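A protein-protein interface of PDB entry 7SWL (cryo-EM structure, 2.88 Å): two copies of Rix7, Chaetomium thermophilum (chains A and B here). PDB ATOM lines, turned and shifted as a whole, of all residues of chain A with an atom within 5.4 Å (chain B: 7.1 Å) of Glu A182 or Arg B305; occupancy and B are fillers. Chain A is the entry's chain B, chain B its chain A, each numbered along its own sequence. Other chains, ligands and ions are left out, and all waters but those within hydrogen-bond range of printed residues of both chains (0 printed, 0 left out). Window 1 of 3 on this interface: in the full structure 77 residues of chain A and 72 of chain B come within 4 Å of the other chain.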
ATOM      1  N   LEU A  56       2.484  28.108  14.966  1.00  0.00           N
ATOM      2  CA  LEU A  56       3.903  28.153  15.286  1.00  0.00           C
ATOM      3  C   LEU A  56       4.440  29.536  14.952  1.00  0.00           C
ATOM      4  O   LEU A  56       4.301  30.002  13.816  1.00  0.00           O
ATOM      5  CB  LEU A  56       4.677  27.083  14.517  1.00  0.00           C
ATOM      6  CG  LEU A  56       6.197  27.081  14.695  1.00  0.00           C
ATOM      7  CD1 LEU A  56       6.577  26.677  16.105  1.00  0.00           C
ATOM      8  CD2 LEU A  56       6.855  26.166  13.682  1.00  0.00           C
ATOM      9  N   HIS A  58       7.796  31.852  14.614  1.00  0.00           N
ATOM     10  CA  HIS A  58       9.240  31.789  14.467  1.00  0.00           C
ATOM     11  C   HIS A  58       9.752  33.117  13.935  1.00  0.00           C
ATOM     12  O   HIS A  58       9.015  33.896  13.327  1.00  0.00           O
ATOM     13  CB  HIS A  58       9.675  30.630  13.557  1.00  0.00           C
ATOM     14  CG  HIS A  58       9.261  30.784  12.128  1.00  0.00           C
ATOM     15  ND1 HIS A  58       8.128  30.194  11.613  1.00  0.00           N
ATOM     16  CD2 HIS A  58       9.842  31.443  11.099  1.00  0.00           C
ATOM     17  CE1 HIS A  58       8.022  30.492  10.332  1.00  0.00           C
ATOM     18  NE2 HIS A  58       9.049  31.249   9.994  1.00  0.00           N
ATOM     19  N   GLU A 169      14.218  25.355  12.055  1.00  0.00           N
ATOM     20  CA  GLU A 169      14.843  24.280  11.298  1.00  0.00           C
ATOM     21  C   GLU A 169      15.301  23.125  12.178  1.00  0.00           C
ATOM     22  O   GLU A 169      15.597  22.049  11.649  1.00  0.00           O
ATOM     23  CB  GLU A 169      16.030  24.826  10.503  1.00  0.00           C
ATOM     24  CG  GLU A 169      15.731  26.116   9.757  1.00  0.00           C
ATOM     25  CD  GLU A 169      14.647  25.955   8.706  1.00  0.00           C
ATOM     26  OE1 GLU A 169      14.482  24.835   8.182  1.00  0.00           O
ATOM     27  OE2 GLU A 169      13.959  26.953   8.404  1.00  0.00           O
ATOM     28  N   ARG A 176       6.672  19.619  13.094  1.00  0.00           N
ATOM     29  CA  ARG A 176       6.471  20.887  12.403  1.00  0.00           C
ATOM     30  C   ARG A 176       5.256  20.842  11.485  1.00  0.00           C
ATOM     31  O   ARG A 176       4.622  21.876  11.248  1.00  0.00           O
ATOM     32  CB  ARG A 176       7.722  21.255  11.611  1.00  0.00           C
ATOM     33  CG  ARG A 176       7.677  22.648  11.024  1.00  0.00           C
ATOM     34  CD  ARG A 176       8.966  23.010  10.320  1.00  0.00           C
ATOM     35  NE  ARG A 176       8.961  24.403   9.893  1.00  0.00           N
ATOM     36  CZ  ARG A 176       9.972  25.003   9.281  1.00  0.00           C
ATOM     37  NH1 ARG A 176      11.092  24.359   9.004  1.00  0.00           N
ATOM     38  NH2 ARG A 176       9.856  26.283   8.944  1.00  0.00           N
ATOM     39  N   ARG A 177       4.913  19.663  10.963  1.00  0.00           N
ATOM     40  CA  ARG A 177       3.754  19.553  10.085  1.00  0.00           C
ATOM     41  C   ARG A 177       2.439  19.673  10.841  1.00  0.00           C
ATOM     42  O   ARG A 177       1.416  19.990  10.227  1.00  0.00           O
ATOM     43  CB  ARG A 177       3.781  18.226   9.326  1.00  0.00           C
ATOM     44  CG  ARG A 177       3.260  17.048  10.128  1.00  0.00           C
ATOM     45  CD  ARG A 177       2.404  16.136   9.272  1.00  0.00           C
ATOM     46  NE  ARG A 177       1.687  15.153  10.074  1.00  0.00           N
ATOM     47  CZ  ARG A 177       0.478  15.343  10.584  1.00  0.00           C
ATOM     48  NH1 ARG A 177      -0.182  16.472  10.395  1.00  0.00           N
ATOM     49  NH2 ARG A 177      -0.082  14.375  11.304  1.00  0.00           N
ATOM     50  N   PHE A 179       1.596  21.896  12.945  1.00  0.00           N
ATOM     51  CA  PHE A 179       1.205  23.294  13.060  1.00  0.00           C
ATOM     52  C   PHE A 179       0.700  23.749  11.697  1.00  0.00           C
ATOM     53  O   PHE A 179       1.484  23.908  10.758  1.00  0.00           O
ATOM     54  CB  PHE A 179       2.376  24.145  13.541  1.00  0.00           C
ATOM     55  CG  PHE A 179       2.832  23.810  14.929  1.00  0.00           C
ATOM     56  CD1 PHE A 179       2.222  24.386  16.028  1.00  0.00           C
ATOM     57  CD2 PHE A 179       3.864  22.915  15.137  1.00  0.00           C
ATOM     58  CE1 PHE A 179       2.636  24.080  17.304  1.00  0.00           C
ATOM     59  CE2 PHE A 179       4.282  22.605  16.413  1.00  0.00           C
ATOM     60  CZ  PHE A 179       3.667  23.188  17.498  1.00  0.00           C
ATOM     61  N   SER A 180      -0.615  23.940  11.588  1.00  0.00           N
ATOM     62  CA  SER A 180      -1.202  24.332  10.314  1.00  0.00           C
ATOM     63  C   SER A 180      -0.764  25.727   9.896  1.00  0.00           C
ATOM     64  O   SER A 180      -0.698  26.020   8.697  1.00  0.00           O
ATOM     65  CB  SER A 180      -2.725  24.260  10.397  1.00  0.00           C
ATOM     66  OG  SER A 180      -3.225  25.169  11.359  1.00  0.00           O
ATOM     67  N   VAL A 181      -0.460  26.592  10.858  1.00  0.00           N
ATOM     68  CA  VAL A 181      -0.084  27.975  10.594  1.00  0.00           C
ATOM     69  C   VAL A 181       1.325  28.204  11.114  1.00  0.00           C
ATOM     70  O   VAL A 181       1.625  27.887  12.270  1.00  0.00           O
ATOM     71  CB  VAL A 181      -1.066  28.964  11.248  1.00  0.00           C
ATOM     72  CG1 VAL A 181      -0.689  30.388  10.896  1.00  0.00           C
ATOM     73  CG2 VAL A 181      -2.485  28.660  10.818  1.00  0.00           C
ATOM     74  N   GLU A 182       2.186  28.747  10.259  1.00  0.00           N
ATOM     75  CA  GLU A 182       3.510  29.210  10.649  1.00  0.00           C
ATOM     76  C   GLU A 182       3.614  30.690  10.322  1.00  0.00           C
ATOM     77  O   GLU A 182       3.391  31.092   9.176  1.00  0.00           O
ATOM     78  CB  GLU A 182       4.611  28.430   9.932  1.00  0.00           C
ATOM     79  CG  GLU A 182       4.659  26.960  10.287  1.00  0.00           C
ATOM     80  CD  GLU A 182       5.866  26.263   9.699  1.00  0.00           C
ATOM     81  OE1 GLU A 182       6.738  26.953   9.133  1.00  0.00           O
ATOM     82  OE2 GLU A 182       5.943  25.024   9.804  1.00  0.00           O
ATOM     83  N   ILE A 183       3.953  31.495  11.323  1.00  0.00           N
ATOM     84  CA  ILE A 183       4.012  32.944  11.184  1.00  0.00           C
ATOM     85  C   ILE A 183       5.455  33.384  11.367  1.00  0.00           C
ATOM     86  O   ILE A 183       6.057  33.136  12.418  1.00  0.00           O
ATOM     87  CB  ILE A 183       3.089  33.651  12.187  1.00  0.00           C
ATOM     88  CG1 ILE A 183       1.628  33.375  11.834  1.00  0.00           C
ATOM     89  CG2 ILE A 183       3.374  35.138  12.213  1.00  0.00           C
ATOM     90  CD1 ILE A 183       0.650  34.248  12.564  1.00  0.00           C
ATOM     91  N   ASP A 184       6.003  34.041  10.350  1.00  0.00           N
ATOM     92  CA  ASP A 184       7.379  34.522  10.380  1.00  0.00           C
ATOM     93  C   ASP A 184       7.373  35.977  10.833  1.00  0.00           C
ATOM     94  O   ASP A 184       6.875  36.854  10.121  1.00  0.00           O
ATOM     95  CB  ASP A 184       8.030  34.372   9.009  1.00  0.00           C
ATOM     96  CG  ASP A 184       9.526  34.595   9.044  1.00  0.00           C
ATOM     97  OD1 ASP A 184      10.074  34.801  10.147  1.00  0.00           O
ATOM     98  OD2 ASP A 184      10.156  34.564   7.968  1.00  0.00           O
ATOM     99  N   ASP B 226      -2.447  18.017   4.911  1.00  0.00           N
ATOM    100  CA  ASP B 226      -2.394  19.320   4.255  1.00  0.00           C
ATOM    101  C   ASP B 226      -3.739  19.688   3.647  1.00  0.00           C
ATOM    102  O   ASP B 226      -4.170  20.843   3.728  1.00  0.00           O
ATOM    103  CB  ASP B 226      -1.304  19.327   3.186  1.00  0.00           C
ATOM    104  CG  ASP B 226       0.080  19.130   3.763  1.00  0.00           C
ATOM    105  OD1 ASP B 226       0.269  19.412   4.964  1.00  0.00           O
ATOM    106  OD2 ASP B 226       0.983  18.699   3.017  1.00  0.00           O
ATOM    107  N   TYR B 229      -5.943  21.023   6.241  1.00  0.00           N
ATOM    108  CA  TYR B 229      -5.694  22.428   6.545  1.00  0.00           C
ATOM    109  C   TYR B 229      -6.363  23.338   5.524  1.00  0.00           C
ATOM    110  O   TYR B 229      -6.838  24.424   5.871  1.00  0.00           O
ATOM    111  CB  TYR B 229      -4.191  22.704   6.595  1.00  0.00           C
ATOM    112  CG  TYR B 229      -3.429  21.894   7.619  1.00  0.00           C
ATOM    113  CD1 TYR B 229      -4.054  21.402   8.754  1.00  0.00           C
ATOM    114  CD2 TYR B 229      -2.080  21.624   7.447  1.00  0.00           C
ATOM    115  CE1 TYR B 229      -3.357  20.663   9.687  1.00  0.00           C
ATOM    116  CE2 TYR B 229      -1.375  20.886   8.372  1.00  0.00           C
ATOM    117  CZ  TYR B 229      -2.018  20.409   9.491  1.00  0.00           C
ATOM    118  OH  TYR B 229      -1.319  19.672  10.417  1.00  0.00           O
ATOM    119  N   LEU B 298      -3.023  30.123   1.497  1.00  0.00           N
ATOM    120  CA  LEU B 298      -2.642  30.289   2.894  1.00  0.00           C
ATOM    121  C   LEU B 298      -2.009  29.039   3.488  1.00  0.00           C
ATOM    122  O   LEU B 298      -1.295  29.142   4.491  1.00  0.00           O
ATOM    123  CB  LEU B 298      -3.859  30.683   3.731  1.00  0.00           C
ATOM    124  CG  LEU B 298      -4.467  32.057   3.466  1.00  0.00           C
ATOM    125  CD1 LEU B 298      -5.622  32.303   4.416  1.00  0.00           C
ATOM    126  CD2 LEU B 298      -3.411  33.137   3.607  1.00  0.00           C
ATOM    127  N   VAL B 299      -2.248  27.870   2.904  1.00  0.00           N
ATOM    128  CA  VAL B 299      -1.768  26.608   3.452  1.00  0.00           C
ATOM    129  C   VAL B 299      -0.474  26.232   2.746  1.00  0.00           C
ATOM    130  O   VAL B 299      -0.453  26.045   1.524  1.00  0.00           O
ATOM    131  CB  VAL B 299      -2.816  25.495   3.306  1.00  0.00           C
ATOM    132  CG1 VAL B 299      -2.226  24.162   3.729  1.00  0.00           C
ATOM    133  CG2 VAL B 299      -4.042  25.821   4.134  1.00  0.00           C
ATOM    134  N   GLN B 300       0.604  26.119   3.519  1.00  0.00           N
ATOM    135  CA  GLN B 300       1.873  25.635   3.006  1.00  0.00           C
ATOM    136  C   GLN B 300       1.978  24.145   3.280  1.00  0.00           C
ATOM    137  O   GLN B 300       1.935  23.740   4.452  1.00  0.00           O
ATOM    138  CB  GLN B 300       3.035  26.378   3.655  1.00  0.00           C
ATOM    139  CG  GLN B 300       4.417  25.932   3.193  1.00  0.00           C
ATOM    140  CD  GLN B 300       4.832  26.540   1.862  1.00  0.00           C
ATOM    141  OE1 GLN B 300       3.997  26.839   1.009  1.00  0.00           O
ATOM    142  NE2 GLN B 300       6.133  26.728   1.683  1.00  0.00           N
ATOM    143  N   PRO B 301       2.100  23.301   2.259  1.00  0.00           N
ATOM    144  CA  PRO B 301       2.179  21.858   2.503  1.00  0.00           C
ATOM    145  C   PRO B 301       3.424  21.494   3.295  1.00  0.00           C
ATOM    146  O   PRO B 301       4.441  22.189   3.251  1.00  0.00           O
ATOM    147  CB  PRO B 301       2.216  21.261   1.092  1.00  0.00           C
ATOM    148  CG  PRO B 301       2.717  22.363   0.230  1.00  0.00           C
ATOM    149  CD  PRO B 301       2.178  23.624   0.825  1.00  0.00           C
ATOM    150  N   ALA B 302       3.328  20.388   4.036  1.00  0.00           N
ATOM    151  CA  ALA B 302       4.439  19.954   4.876  1.00  0.00           C
ATOM    152  C   ALA B 302       5.683  19.644   4.057  1.00  0.00           C
ATOM    153  O   ALA B 302       6.804  19.754   4.568  1.00  0.00           O
ATOM    154  CB  ALA B 302       4.029  18.732   5.695  1.00  0.00           C
ATOM    155  N   SER B 303       5.514  19.251   2.795  1.00  0.00           N
ATOM    156  CA  SER B 303       6.663  18.969   1.945  1.00  0.00           C
ATOM    157  C   SER B 303       7.444  20.226   1.586  1.00  0.00           C
ATOM    158  O   SER B 303       8.625  20.127   1.241  1.00  0.00           O
ATOM    159  CB  SER B 303       6.211  18.256   0.671  1.00  0.00           C
ATOM    160  OG  SER B 303       5.227  19.010  -0.014  1.00  0.00           O
ATOM    161  N   LYS B 304       6.818  21.399   1.663  1.00  0.00           N
ATOM    162  CA  LYS B 304       7.461  22.654   1.302  1.00  0.00           C
ATOM    163  C   LYS B 304       7.834  23.500   2.512  1.00  0.00           C
ATOM    164  O   LYS B 304       8.131  24.688   2.354  1.00  0.00           O
ATOM    165  CB  LYS B 304       6.560  23.458   0.367  1.00  0.00           C
ATOM    166  CG  LYS B 304       6.339  22.813  -0.980  1.00  0.00           C
ATOM    167  CD  LYS B 304       5.623  23.765  -1.907  1.00  0.00           C
ATOM    168  CE  LYS B 304       6.409  25.053  -2.073  1.00  0.00           C
ATOM    169  NZ  LYS B 304       5.687  26.034  -2.925  1.00  0.00           N
ATOM    170  N   ARG B 305       7.822  22.924   3.714  1.00  0.00           N
ATOM    171  CA  ARG B 305       8.177  23.696   4.899  1.00  0.00           C
ATOM    172  C   ARG B 305       9.652  24.074   4.906  1.00  0.00           C
ATOM    173  O   ARG B 305      10.008  25.156   5.383  1.00  0.00           O
ATOM    174  CB  ARG B 305       7.827  22.912   6.162  1.00  0.00           C
ATOM    175  CG  ARG B 305       6.340  22.717   6.383  1.00  0.00           C
ATOM    176  CD  ARG B 305       5.637  24.035   6.641  1.00  0.00           C
ATOM    177  NE  ARG B 305       4.200  23.859   6.809  1.00  0.00           N
ATOM    178  CZ  ARG B 305       3.603  23.629   7.969  1.00  0.00           C
ATOM    179  NH1 ARG B 305       4.289  23.545   9.095  1.00  0.00           N
ATOM    180  NH2 ARG B 305       2.282  23.480   8.000  1.00  0.00           N
ATOM    181  N   GLU B 306      10.517  23.207   4.388  1.00  0.00           N
ATOM    182  CA  GLU B 306      11.955  23.427   4.434  1.00  0.00           C
ATOM    183  C   GLU B 306      12.591  22.991   3.123  1.00  0.00           C
ATOM    184  O   GLU B 306      12.244  21.942   2.576  1.00  0.00           O
ATOM    185  CB  GLU B 306      12.587  22.661   5.602  1.00  0.00           C
ATOM    186  CG  GLU B 306      14.093  22.806   5.710  1.00  0.00           C
ATOM    187  CD  GLU B 306      14.686  21.899   6.769  1.00  0.00           C
ATOM    188  OE1 GLU B 306      13.988  20.961   7.204  1.00  0.00           O
ATOM    189  OE2 GLU B 306      15.849  22.124   7.166  1.00  0.00           O
ATOM    190  N   GLY B 307      13.524  23.801   2.627  1.00  0.00           N
ATOM    191  CA  GLY B 307      14.337  23.438   1.487  1.00  0.00           C
ATOM    192  C   GLY B 307      13.923  24.030   0.158  1.00  0.00           C
ATOM    193  O   GLY B 307      14.595  23.771  -0.846  1.00  0.00           O
ATOM    194  N   PHE B 308      12.854  24.816   0.116  1.00  0.00           N
ATOM    195  CA  PHE B 308      12.345  25.382  -1.124  1.00  0.00           C
ATOM    196  C   PHE B 308      12.520  26.893  -1.121  1.00  0.00           C
ATOM    197  O   PHE B 308      12.356  27.546  -0.087  1.00  0.00           O
ATOM    198  CB  PHE B 308      10.872  25.021  -1.326  1.00  0.00           C
ATOM    199  CG  PHE B 308      10.652  23.597  -1.738  1.00  0.00           C
ATOM    200  CD1 PHE B 308      10.739  22.573  -0.813  1.00  0.00           C
ATOM    201  CD2 PHE B 308      10.362  23.280  -3.052  1.00  0.00           C
ATOM    202  CE1 PHE B 308      10.542  21.263  -1.190  1.00  0.00           C
ATOM    203  CE2 PHE B 308      10.165  21.971  -3.434  1.00  0.00           C
ATOM    204  CZ  PHE B 308      10.254  20.962  -2.502  1.00  0.00           C
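The backbone carbonyl oxygen (O) of Arg A177 lies within hydrogen-bond range of the side-chain hydroxyl (OH) of Tyr B229. The backbone carbonyl oxygen of Arg A176 sits at hydrogen-bond distance from the guanidinium group of Arg B305, 2.7 Å away. NH2 of Arg B305 sits at hydrogen-bond distance from O of Phe A179 (2.9 Å). The side-chain carboxylate of Glu A182 is in salt-bridge range of the guanidinium group of Arg B305 (3.7 Å). OE1 of Glu A169 sits close to OE2 of Glu B306, at 3.2 Å.
The side-chain carboxylate of Asp B226 sits at hydrogen-bond distance from the backbone NH of Ala B302, 3.1 Å away. O of Gln B300 sits at hydrogen-bond distance from NE of Arg B305 (3.3 Å). The guanidinium group of Arg A176 is in salt-bridge range of the side-chain carboxylate of Glu A169 (3.5 Å). NE of Arg A176 is in salt-bridge range of OE2 of Glu A182 (3.1 Å).
CB of Arg A177 touches CB of Ala B302 (3.7 Å). Ser A180 touches Tyr B229. Ser A180 touches Arg B305 (O to NH2, 3.98 Å).
Of the printed residues of chain B, Glu A169 touches Glu B306. Of the printed residues of chain B, Arg A177 touches Tyr B229 (2.8 Å) and Ala B302 (3.7 Å). Of the printed residues of chain B, Phe A179 touches Arg B305. Of the printed residues of chain B, Ser A180 touches Tyr B229 and Arg B305. Of the printed residues of chain A, Ala B302 touches Arg A177 (3.7 Å). Ser B303 touches none of the printed residues of chain A. Lys B304 touches none of the printed residues of chain A. Of chain A, only Arg A176, Phe A179, Ser A180 and Glu A182 come within 4 Å of Arg B305. The nearest printed residue of chain B that does not touch Arg A176 is Glu B306 (4.1 Å).
Of the 11 printed residues of chain A, 6 touch a printed residue of chain B. Among the printed residues, 8 pairs touch across the chains. Among the printed residues, Asp or Glu carboxylates within 4 Å of a Lys or Arg side-chain nitrogen of the other chain: Glu A182 with Arg B305 (2.3 Å).
No position is printed for both chains.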
